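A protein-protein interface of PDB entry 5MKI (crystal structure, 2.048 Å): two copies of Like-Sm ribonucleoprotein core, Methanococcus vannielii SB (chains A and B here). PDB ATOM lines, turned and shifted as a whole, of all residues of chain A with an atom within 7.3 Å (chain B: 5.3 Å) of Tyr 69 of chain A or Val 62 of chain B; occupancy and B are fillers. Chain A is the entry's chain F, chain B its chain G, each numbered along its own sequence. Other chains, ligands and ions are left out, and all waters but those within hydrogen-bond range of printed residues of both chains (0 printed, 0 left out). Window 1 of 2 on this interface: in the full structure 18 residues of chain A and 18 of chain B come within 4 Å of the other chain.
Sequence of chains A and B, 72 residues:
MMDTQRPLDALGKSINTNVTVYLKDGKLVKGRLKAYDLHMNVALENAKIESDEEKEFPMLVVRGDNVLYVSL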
ATOM      1  N   PRO A   7     -28.186  -7.727  14.717  1.00  0.00           N
ATOM      2  CA  PRO A   7     -27.770  -6.425  15.264  1.00  0.00           C
ATOM      3  C   PRO A   7     -28.518  -5.233  14.677  1.00  0.00           C
ATOM      4  O   PRO A   7     -28.774  -4.264  15.406  1.00  0.00           O
ATOM      5  CB  PRO A   7     -26.266  -6.382  14.948  1.00  0.00           C
ATOM      6  CG  PRO A   7     -26.068  -7.410  13.817  1.00  0.00           C
ATOM      7  CD  PRO A   7     -27.063  -8.478  14.122  1.00  0.00           C
ATOM      8  N   LEU A   8     -28.895  -5.266  13.393  1.00  0.00           N
ATOM      9  CA  LEU A   8     -29.549  -4.099  12.803  1.00  0.00           C
ATOM     10  C   LEU A   8     -30.984  -3.901  13.296  1.00  0.00           C
ATOM     11  O   LEU A   8     -31.547  -2.825  13.064  1.00  0.00           O
ATOM     12  CB  LEU A   8     -29.529  -4.189  11.264  1.00  0.00           C
ATOM     13  CG  LEU A   8     -28.148  -4.373  10.597  1.00  0.00           C
ATOM     14  CD1 LEU A   8     -28.225  -4.219   9.069  1.00  0.00           C
ATOM     15  CD2 LEU A   8     -27.111  -3.407  11.159  1.00  0.00           C
ATOM     16  N   THR A  20     -26.940   9.361  15.592  1.00  0.00           N
ATOM     17  CA  THR A  20     -25.719   9.908  15.005  1.00  0.00           C
ATOM     18  C   THR A  20     -25.023   8.822  14.193  1.00  0.00           C
ATOM     19  O   THR A  20     -24.704   7.746  14.722  1.00  0.00           O
ATOM     20  CB  THR A  20     -24.782  10.463  16.082  1.00  0.00           C
ATOM     21  OG1 THR A  20     -25.480  11.445  16.845  1.00  0.00           O
ATOM     22  CG2 THR A  20     -23.539  11.113  15.451  1.00  0.00           C
ATOM     23  N   VAL A  21     -24.784   9.108  12.920  1.00  0.00           N
ATOM     24  CA  VAL A  21     -24.141   8.178  12.002  1.00  0.00           C
ATOM     25  C   VAL A  21     -22.709   8.644  11.808  1.00  0.00           C
ATOM     26  O   VAL A  21     -22.463   9.698  11.211  1.00  0.00           O
ATOM     27  CB  VAL A  21     -24.874   8.091  10.656  1.00  0.00           C
ATOM     28  CG1 VAL A  21     -24.218   6.996   9.770  1.00  0.00           C
ATOM     29  CG2 VAL A  21     -26.330   7.792  10.864  1.00  0.00           C
ATOM     30  N   TYR A  22     -21.767   7.856  12.303  1.00  0.00           N
ATOM     31  CA  TYR A  22     -20.351   8.138  12.138  1.00  0.00           C
ATOM     32  C   TYR A  22     -19.886   7.563  10.808  1.00  0.00           C
ATOM     33  O   TYR A  22     -20.129   6.390  10.517  1.00  0.00           O
ATOM     34  CB  TYR A  22     -19.554   7.532  13.301  1.00  0.00           C
ATOM     35  CG  TYR A  22     -19.788   8.217  14.628  1.00  0.00           C
ATOM     36  CD1 TYR A  22     -20.953   7.995  15.353  1.00  0.00           C
ATOM     37  CD2 TYR A  22     -18.840   9.083  15.162  1.00  0.00           C
ATOM     38  CE1 TYR A  22     -21.169   8.625  16.578  1.00  0.00           C
ATOM     39  CE2 TYR A  22     -19.037   9.704  16.383  1.00  0.00           C
ATOM     40  CZ  TYR A  22     -20.204   9.474  17.086  1.00  0.00           C
ATOM     41  OH  TYR A  22     -20.404  10.105  18.295  1.00  0.00           O
ATOM     42  N   LEU A  23     -19.241   8.389   9.996  1.00  0.00           N
ATOM     43  CA  LEU A  23     -18.773   7.954   8.689  1.00  0.00           C
ATOM     44  C   LEU A  23     -17.288   7.619   8.740  1.00  0.00           C
ATOM     45  O   LEU A  23     -16.557   8.102   9.603  1.00  0.00           O
ATOM     46  CB  LEU A  23     -19.034   9.033   7.631  1.00  0.00           C
ATOM     47  CG  LEU A  23     -20.510   9.447   7.576  1.00  0.00           C
ATOM     48  CD1 LEU A  23     -20.733  10.481   6.488  1.00  0.00           C
ATOM     49  CD2 LEU A  23     -21.395   8.217   7.381  1.00  0.00           C
ATOM     50  N   LYS A  24     -16.848   6.800   7.779  1.00  0.00           N
ATOM     51  CA  LYS A  24     -15.445   6.383   7.734  1.00  0.00           C
ATOM     52  C   LYS A  24     -14.507   7.583   7.711  1.00  0.00           C
ATOM     53  O   LYS A  24     -13.451   7.565   8.355  1.00  0.00           O
ATOM     54  CB  LYS A  24     -15.184   5.502   6.515  1.00  0.00           C
ATOM     55  CG  LYS A  24     -15.770   4.098   6.579  1.00  0.00           C
ATOM     56  CD  LYS A  24     -15.394   3.318   5.308  1.00  0.00           C
ATOM     57  CE  LYS A  24     -15.854   1.869   5.363  1.00  0.00           C
ATOM     58  NZ  LYS A  24     -17.187   1.692   6.028  1.00  0.00           N
ATOM     59  N   LYS A  27     -16.780  12.130   9.442  1.00  0.00           N
ATOM     60  CA  LYS A  27     -17.961  12.965   9.600  1.00  0.00           C
ATOM     61  C   LYS A  27     -18.911  12.359  10.626  1.00  0.00           C
ATOM     62  O   LYS A  27     -18.972  11.140  10.811  1.00  0.00           O
ATOM     63  CB  LYS A  27     -18.687  13.144   8.269  1.00  0.00           C
ATOM     64  CG  LYS A  27     -17.966  14.026   7.261  1.00  0.00           C
ATOM     65  CD  LYS A  27     -18.872  14.322   6.051  1.00  0.00           C
ATOM     66  CE  LYS A  27     -18.086  14.916   4.885  1.00  0.00           C
ATOM     67  NZ  LYS A  27     -17.027  13.984   4.373  1.00  0.00           N
ATOM     68  N   MET A  40     -27.056  -1.282   5.733  1.00  0.00           N
ATOM     69  CA  MET A  40     -26.934  -0.083   6.547  1.00  0.00           C
ATOM     70  C   MET A  40     -26.998   1.198   5.707  1.00  0.00           C
ATOM     71  O   MET A  40     -26.427   2.222   6.083  1.00  0.00           O
ATOM     72  CB  MET A  40     -25.662  -0.144   7.415  1.00  0.00           C
ATOM     73  CG  MET A  40     -25.675  -1.359   8.334  1.00  0.00           C
ATOM     74  SD  MET A  40     -24.358  -1.440   9.582  1.00  0.00           S
ATOM     75  CE  MET A  40     -24.352   0.265  10.097  1.00  0.00           C
ATOM     76  N   ASN A  66     -20.293   3.699   3.630  1.00  0.00           N
ATOM     77  CA  ASN A  66     -19.538   4.774   4.266  1.00  0.00           C
ATOM     78  C   ASN A  66     -19.621   4.752   5.788  1.00  0.00           C
ATOM     79  O   ASN A  66     -18.976   5.583   6.439  1.00  0.00           O
ATOM     80  CB  ASN A  66     -20.033   6.130   3.767  1.00  0.00           C
ATOM     81  CG  ASN A  66     -19.958   6.244   2.261  1.00  0.00           C
ATOM     82  OD1 ASN A  66     -18.866   6.271   1.688  1.00  0.00           O
ATOM     83  ND2 ASN A  66     -21.115   6.284   1.614  1.00  0.00           N
ATOM     84  N   VAL A  67     -20.409   3.846   6.372  1.00  0.00           N
ATOM     85  CA  VAL A  67     -20.714   3.936   7.794  1.00  0.00           C
ATOM     86  C   VAL A  67     -19.602   3.276   8.597  1.00  0.00           C
ATOM     87  O   VAL A  67     -19.100   2.205   8.238  1.00  0.00           O
ATOM     88  CB  VAL A  67     -22.081   3.301   8.094  1.00  0.00           C
ATOM     89  CG1 VAL A  67     -22.334   3.215   9.636  1.00  0.00           C
ATOM     90  CG2 VAL A  67     -23.182   4.103   7.396  1.00  0.00           C
ATOM     91  N   LEU A  68     -19.191   3.942   9.674  1.00  0.00           N
ATOM     92  CA  LEU A  68     -18.337   3.341  10.694  1.00  0.00           C
ATOM     93  C   LEU A  68     -19.198   2.667  11.768  1.00  0.00           C
ATOM     94  O   LEU A  68     -19.153   1.443  11.937  1.00  0.00           O
ATOM     95  CB  LEU A  68     -17.419   4.426  11.276  1.00  0.00           C
ATOM     96  CG  LEU A  68     -16.190   4.051  12.109  1.00  0.00           C
ATOM     97  CD1 LEU A  68     -15.053   3.467  11.241  1.00  0.00           C
ATOM     98  CD2 LEU A  68     -15.714   5.302  12.819  1.00  0.00           C
ATOM     99  N   TYR A  69     -20.040   3.447  12.446  1.00  0.00           N
ATOM    100  CA  TYR A  69     -21.025   2.906  13.381  1.00  0.00           C
ATOM    101  C   TYR A  69     -22.111   3.948  13.591  1.00  0.00           C
ATOM    102  O   TYR A  69     -21.940   5.126  13.268  1.00  0.00           O
ATOM    103  CB  TYR A  69     -20.407   2.511  14.732  1.00  0.00           C
ATOM    104  CG  TYR A  69     -19.295   3.415  15.206  1.00  0.00           C
ATOM    105  CD1 TYR A  69     -19.538   4.733  15.557  1.00  0.00           C
ATOM    106  CD2 TYR A  69     -17.996   2.936  15.312  1.00  0.00           C
ATOM    107  CE1 TYR A  69     -18.514   5.556  16.001  1.00  0.00           C
ATOM    108  CE2 TYR A  69     -16.963   3.744  15.751  1.00  0.00           C
ATOM    109  CZ  TYR A  69     -17.218   5.051  16.089  1.00  0.00           C
ATOM    110  OH  TYR A  69     -16.171   5.844  16.530  1.00  0.00           O
ATOM    111  N   VAL A  70     -23.224   3.498  14.163  1.00  0.00           N
ATOM    112  CA  VAL A  70     -24.376   4.347  14.435  1.00  0.00           C
ATOM    113  C   VAL A  70     -24.610   4.371  15.941  1.00  0.00           C
ATOM    114  O   VAL A  70     -24.738   3.314  16.572  1.00  0.00           O
ATOM    115  CB  VAL A  70     -25.633   3.857  13.693  1.00  0.00           C
ATOM    116  CG1 VAL A  70     -26.825   4.736  14.038  1.00  0.00           C
ATOM    117  CG2 VAL A  70     -25.393   3.863  12.182  1.00  0.00           C
ATOM    118  N   SER A  71     -24.669   5.578  16.508  1.00  0.00           N
ATOM    119  CA  SER A  71     -24.976   5.776  17.921  1.00  0.00           C
ATOM    120  C   SER A  71     -26.478   5.970  18.078  1.00  0.00           C
ATOM    121  O   SER A  71     -27.057   6.894  17.491  1.00  0.00           O
ATOM    122  CB  SER A  71     -24.223   6.979  18.481  1.00  0.00           C
ATOM    123  OG  SER A  71     -24.236   6.952  19.896  1.00  0.00           O
ATOM    124  N   VAL B  21     -13.730  -4.413  20.236  1.00  0.00           N
ATOM    125  CA  VAL B  21     -13.703  -4.459  18.779  1.00  0.00           C
ATOM    126  C   VAL B  21     -12.610  -3.514  18.295  1.00  0.00           C
ATOM    127  O   VAL B  21     -12.668  -2.304  18.546  1.00  0.00           O
ATOM    128  CB  VAL B  21     -15.069  -4.088  18.176  1.00  0.00           C
ATOM    129  CG1 VAL B  21     -15.024  -4.197  16.677  1.00  0.00           C
ATOM    130  CG2 VAL B  21     -16.173  -4.988  18.744  1.00  0.00           C
ATOM    131  N   LEU B  23     -10.920  -1.712  15.206  1.00  0.00           N
ATOM    132  CA  LEU B  23     -11.272  -1.238  13.875  1.00  0.00           C
ATOM    133  C   LEU B  23     -10.016  -0.975  13.061  1.00  0.00           C
ATOM    134  O   LEU B  23      -8.920  -0.830  13.606  1.00  0.00           O
ATOM    135  CB  LEU B  23     -12.115   0.042  13.957  1.00  0.00           C
ATOM    136  CG  LEU B  23     -13.376  -0.092  14.808  1.00  0.00           C
ATOM    137  CD1 LEU B  23     -14.264   1.164  14.670  1.00  0.00           C
ATOM    138  CD2 LEU B  23     -14.137  -1.362  14.426  1.00  0.00           C
ATOM    139  N   LYS B  27      -9.084   2.481  16.114  1.00  0.00           N
ATOM    140  CA  LYS B  27      -9.970   2.627  17.259  1.00  0.00           C
ATOM    141  C   LYS B  27     -10.188   1.292  17.961  1.00  0.00           C
ATOM    142  O   LYS B  27     -10.238   0.232  17.333  1.00  0.00           O
ATOM    143  CB  LYS B  27     -11.322   3.195  16.827  1.00  0.00           C
ATOM    144  CG  LYS B  27     -11.311   4.678  16.508  1.00  0.00           C
ATOM    145  CD  LYS B  27     -12.729   5.174  16.264  1.00  0.00           C
ATOM    146  CE  LYS B  27     -12.723   6.609  15.769  1.00  0.00           C
ATOM    147  NZ  LYS B  27     -12.314   6.713  14.325  1.00  0.00           N
ATOM    148  N   VAL B  29     -13.133  -0.223  20.405  1.00  0.00           N
ATOM    149  CA  VAL B  29     -14.493  -0.025  20.889  1.00  0.00           C
ATOM    150  C   VAL B  29     -14.803  -1.160  21.850  1.00  0.00           C
ATOM    151  O   VAL B  29     -14.811  -2.334  21.455  1.00  0.00           O
ATOM    152  CB  VAL B  29     -15.510   0.016  19.737  1.00  0.00           C
ATOM    153  CG1 VAL B  29     -16.839   0.533  20.213  1.00  0.00           C
ATOM    154  CG2 VAL B  29     -14.986   0.871  18.578  1.00  0.00           C
ATOM    155  N   MET B  40     -20.213  -9.673  10.554  1.00  0.00           N
ATOM    156  CA  MET B  40     -19.541  -9.115  11.717  1.00  0.00           C
ATOM    157  C   MET B  40     -19.991  -7.695  12.037  1.00  0.00           C
ATOM    158  O   MET B  40     -19.242  -6.946  12.675  1.00  0.00           O
ATOM    159  CB  MET B  40     -18.013  -9.187  11.568  1.00  0.00           C
ATOM    160  CG  MET B  40     -17.518 -10.631  11.433  1.00  0.00           C
ATOM    161  SD  MET B  40     -15.721 -10.863  11.585  1.00  0.00           S
ATOM    162  CE  MET B  40     -15.394  -9.857  13.036  1.00  0.00           C
ATOM    163  N   ASN B  41     -21.194  -7.290  11.595  1.00  0.00           N
ATOM    164  CA  ASN B  41     -21.884  -6.202  12.284  1.00  0.00           C
ATOM    165  C   ASN B  41     -22.137  -6.625  13.726  1.00  0.00           C
ATOM    166  O   ASN B  41     -22.560  -7.752  13.986  1.00  0.00           O
ATOM    167  CB  ASN B  41     -23.231  -5.860  11.612  1.00  0.00           C
ATOM    168  CG  ASN B  41     -23.095  -5.519  10.127  1.00  0.00           C
ATOM    169  OD1 ASN B  41     -22.193  -4.785   9.715  1.00  0.00           O
ATOM    170  ND2 ASN B  41     -23.986  -6.069   9.323  1.00  0.00           N
ATOM    171  N   VAL B  42     -21.913  -5.713  14.671  1.00  0.00           N
ATOM    172  CA  VAL B  42     -22.188  -6.012  16.073  1.00  0.00           C
ATOM    173  C   VAL B  42     -22.971  -4.877  16.706  1.00  0.00           C
ATOM    174  O   VAL B  42     -22.800  -3.705  16.358  1.00  0.00           O
ATOM    175  CB  VAL B  42     -20.896  -6.276  16.888  1.00  0.00           C
ATOM    176  CG1 VAL B  42     -20.196  -7.498  16.374  1.00  0.00           C
ATOM    177  CG2 VAL B  42     -19.973  -5.058  16.831  1.00  0.00           C
ATOM    178  N   ALA B  43     -23.822  -5.235  17.667  1.00  0.00           N
ATOM    179  CA  ALA B  43     -24.499  -4.267  18.520  1.00  0.00           C
ATOM    180  C   ALA B  43     -23.839  -4.289  19.896  1.00  0.00           C
ATOM    181  O   ALA B  43     -23.857  -5.321  20.581  1.00  0.00           O
ATOM    182  CB  ALA B  43     -25.995  -4.564  18.630  1.00  0.00           C
ATOM    183  N   LEU B  44     -23.268  -3.154  20.287  1.00  0.00           N
ATOM    184  CA  LEU B  44     -22.570  -2.984  21.557  1.00  0.00           C
ATOM    185  C   LEU B  44     -23.363  -2.034  22.453  1.00  0.00           C
ATOM    186  O   LEU B  44     -23.632  -0.889  22.070  1.00  0.00           O
ATOM    187  CB  LEU B  44     -21.171  -2.435  21.320  1.00  0.00           C
ATOM    188  CG  LEU B  44     -20.336  -3.351  20.432  1.00  0.00           C
ATOM    189  CD1 LEU B  44     -19.048  -2.642  20.088  1.00  0.00           C
ATOM    190  CD2 LEU B  44     -20.089  -4.676  21.155  1.00  0.00           C
ATOM    191  N   ILE B  49     -15.039   4.253  23.595  1.00  0.00           N
ATOM    192  CA  ILE B  49     -13.898   4.276  22.688  1.00  0.00           C
ATOM    193  C   ILE B  49     -12.681   4.760  23.460  1.00  0.00           C
ATOM    194  O   ILE B  49     -12.731   5.804  24.120  1.00  0.00           O
ATOM    195  CB  ILE B  49     -14.168   5.154  21.457  1.00  0.00           C
ATOM    196  CG1 ILE B  49     -15.409   4.644  20.733  1.00  0.00           C
ATOM    197  CG2 ILE B  49     -12.976   5.132  20.525  1.00  0.00           C
ATOM    198  CD1 ILE B  49     -15.722   5.402  19.487  1.00  0.00           C
ATOM    199  N   LEU B  60     -24.453   1.056  20.324  1.00  0.00           N
ATOM    200  CA  LEU B  60     -23.627   1.332  19.159  1.00  0.00           C
ATOM    201  C   LEU B  60     -23.748   0.158  18.205  1.00  0.00           C
ATOM    202  O   LEU B  60     -23.471  -0.983  18.591  1.00  0.00           O
ATOM    203  CB  LEU B  60     -22.167   1.546  19.568  1.00  0.00           C
ATOM    204  CG  LEU B  60     -21.239   2.385  18.695  1.00  0.00           C
ATOM    205  CD1 LEU B  60     -21.753   3.801  18.518  1.00  0.00           C
ATOM    206  CD2 LEU B  60     -19.824   2.382  19.307  1.00  0.00           C
ATOM    207  N   VAL B  61     -24.151   0.430  16.968  1.00  0.00           N
ATOM    208  CA  VAL B  61     -24.186  -0.592  15.925  1.00  0.00           C
ATOM    209  C   VAL B  61     -23.010  -0.335  14.988  1.00  0.00           C
ATOM    210  O   VAL B  61     -22.970   0.686  14.288  1.00  0.00           O
ATOM    211  CB  VAL B  61     -25.521  -0.604  15.172  1.00  0.00           C
ATOM    212  CG1 VAL B  61     -25.447  -1.563  14.000  1.00  0.00           C
ATOM    213  CG2 VAL B  61     -26.651  -0.993  16.112  1.00  0.00           C
ATOM    214  N   VAL B  62     -22.054  -1.266  14.977  1.00  0.00           N
ATOM    215  CA  VAL B  62     -20.789  -1.118  14.268  1.00  0.00           C
ATOM    216  C   VAL B  62     -20.836  -1.951  12.991  1.00  0.00           C
ATOM    217  O   VAL B  62     -21.163  -3.147  13.030  1.00  0.00           O
ATOM    218  CB  VAL B  62     -19.606  -1.564  15.148  1.00  0.00           C
ATOM    219  CG1 VAL B  62     -18.316  -1.591  14.314  1.00  0.00           C
ATOM    220  CG2 VAL B  62     -19.463  -0.670  16.389  1.00  0.00           C
ATOM    221  N   ARG B  63     -20.484  -1.337  11.868  1.00  0.00           N
ATOM    222  CA  ARG B  63     -20.501  -2.041  10.591  1.00  0.00           C
ATOM    223  C   ARG B  63     -19.294  -2.967  10.472  1.00  0.00           C
ATOM    224  O   ARG B  63     -18.150  -2.529  10.621  1.00  0.00           O
ATOM    225  CB  ARG B  63     -20.533  -1.041   9.433  1.00  0.00           C
ATOM    226  CG  ARG B  63     -21.032  -1.652   8.147  1.00  0.00           C
ATOM    227  CD  ARG B  63     -20.991  -0.667   6.983  1.00  0.00           C
ATOM    228  NE  ARG B  63     -21.943  -1.065   5.950  1.00  0.00           N
ATOM    229  CZ  ARG B  63     -21.617  -1.744   4.852  1.00  0.00           C
ATOM    230  NH1 ARG B  63     -20.353  -2.086   4.634  1.00  0.00           N
ATOM    231  NH2 ARG B  63     -22.552  -2.061   3.963  1.00  0.00           N
ATOM    232  N   GLY B  64     -19.556  -4.241  10.154  1.00  0.00           N
ATOM    233  CA  GLY B  64     -18.514  -5.265  10.194  1.00  0.00           C
ATOM    234  C   GLY B  64     -17.308  -5.018   9.305  1.00  0.00           C
ATOM    235  O   GLY B  64     -16.190  -5.412   9.648  1.00  0.00           O
ATOM    236  N   ASN B  66     -15.569  -2.537   8.872  1.00  0.00           N
ATOM    237  CA  ASN B  66     -14.562  -1.731   9.550  1.00  0.00           C
ATOM    238  C   ASN B  66     -13.750  -2.525  10.565  1.00  0.00           C
ATOM    239  O   ASN B  66     -12.791  -1.979  11.119  1.00  0.00           O
ATOM    240  CB  ASN B  66     -15.214  -0.549  10.292  1.00  0.00           C
ATOM    241  CG  ASN B  66     -16.168   0.258   9.412  1.00  0.00           C
ATOM    242  OD1 ASN B  66     -15.749   0.901   8.450  1.00  0.00           O
ATOM    243  ND2 ASN B  66     -17.439   0.247   9.761  1.00  0.00           N
ATOM    244  N   VAL B  67     -14.105  -3.787  10.812  1.00  0.00           N
ATOM    245  CA  VAL B  67     -13.551  -4.547  11.934  1.00  0.00           C
ATOM    246  C   VAL B  67     -12.206  -5.167  11.561  1.00  0.00           C
ATOM    247  O   VAL B  67     -12.066  -5.811  10.511  1.00  0.00           O
ATOM    248  CB  VAL B  67     -14.543  -5.629  12.387  1.00  0.00           C
ATOM    249  CG1 VAL B  67     -13.855  -6.622  13.350  1.00  0.00           C
ATOM    250  CG2 VAL B  67     -15.732  -4.980  13.054  1.00  0.00           C
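Among the printed residues, merely in contact across the chains: Pro 7 of chain A with Asn 41 of chain B, Pro 7 of chain A with Ala 43 of chain B, Pro 7 of chain A with Val 61 of chain B, Leu 8 of chain A with Val 61 of chain B, Met 40 of chain A with Asn 41 of chain B, Met 40 of chain A with Arg 63 of chain B, Val 67 of chain A with Arg 63 of chain B, Leu 68 of chain A with Lys 27 of chain B, Leu 68 of chain A with Val 62 of chain B, Tyr 69 of chain A with Leu 23 of chain B, Tyr 69 of chain A with Lys 27 of chain B, Tyr 69 of chain A with Ile 49 of chain B, Tyr 69 of chain A with Leu 60 of chain B, Tyr 69 of chain A with Val 61 of chain B, Tyr 69 of chain A with Val 62 of chain B, Val 70 of chain A with Leu 60 of chain B and Ser 71 of chain A with Leu 60 of chain B.
The backbone carbonyl oxygen of Leu 68 of chain A lies within hydrogen-bond range of the backbone NH of Arg 63 of chain B (3.1 Å).
The backbone carbonyl oxygen (O) of Val 67 of chain A sits at hydrogen-bond distance from the side-chain amide nitrogen (ND2) of Asn 66 of chain B, 3.0 Å away.
OD1 of Asn 66 of chain B lies within hydrogen-bond range of NZ of Lys 24 of chain A (2.9 Å).
The backbone carbonyl oxygen (O) of Leu 68 of chain A is in hydrogen-bond range of the side-chain amide nitrogen (ND2) of Asn 66 of chain B (3.0 Å).
The backbone NH of Val 70 of chain A sits at hydrogen-bond distance from the backbone carbonyl oxygen of Val 61 of chain B, 2.8 Å away.
The backbone carbonyl oxygen (O) of Asn 66 of chain A sits at hydrogen-bond distance from the backbone NH (N) of Lys 24 of chain A (2.8 Å).
The backbone carbonyl oxygen of Val 42 of chain B sits at hydrogen-bond distance from the backbone NH of Val 62 of chain B.
The backbone carbonyl oxygen of Val 67 of chain A lies within hydrogen-bond range of the side-chain amino group of Lys 24 of chain A (3.0 Å).
The side-chain amide oxygen of Asn 41 of chain B sits at hydrogen-bond distance from the backbone NH of Gly 64 of chain B (2.7 Å).
The backbone NH (N) of Ser 71 of chain A lies within hydrogen-bond range of the backbone carbonyl oxygen (O) of Thr 20 of chain A (2.8 Å).
O of Tyr 22 of chain A is in hydrogen-bond range of N of Leu 68 of chain A, at 2.8 Å.
Val 67 of chain A touches Asn 66 of chain B, but with the chains exchanged Asn 66 of chain A does not touch Val 67 of chain B (11.3 Å).
Of the 22 pairs that touch across the chains among the printed residues, none has its exchanged pair printed and touching as well.
Hydrophobic or aromatic side chains of chain A within 4 Å of the printed part of chain B: Pro 7, Leu 8, Met 40, Leu 68 and Tyr 69.
Along chain B the printed residues that touch a printed residue of chain A span positions 23 to 66.
Among the printed residues, 22 pairs touch across the chains.
Of the printed residues of chain B, Met 40 of chain A touches Asn 41 and Arg 63.
Of the printed residues of chain B, Val 67 of chain A touches Arg 63 and Asn 66.
Of the printed residues of chain B, Leu 68 of chain A touches Lys 27, Val 62, Arg 63 and Asn 66.
Printed residues of chain A within 4 Å of Asn 41 of chain B: Pro 7 (3.5 Å) and Met 40 (3.99 Å).
Of the printed residues of chain A, Leu 60 of chain B touches Tyr 69, Val 70 and Ser 71.
Val 62 of chain B touches two residues of chain A.
The nearest residue of chain B that does not touch Tyr 69 of chain A is Val 29 of chain B (4.5 Å).
The nearest residue of chain A that does not touch Val 62 of chain B is Met 40 of chain A (4.9 Å).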
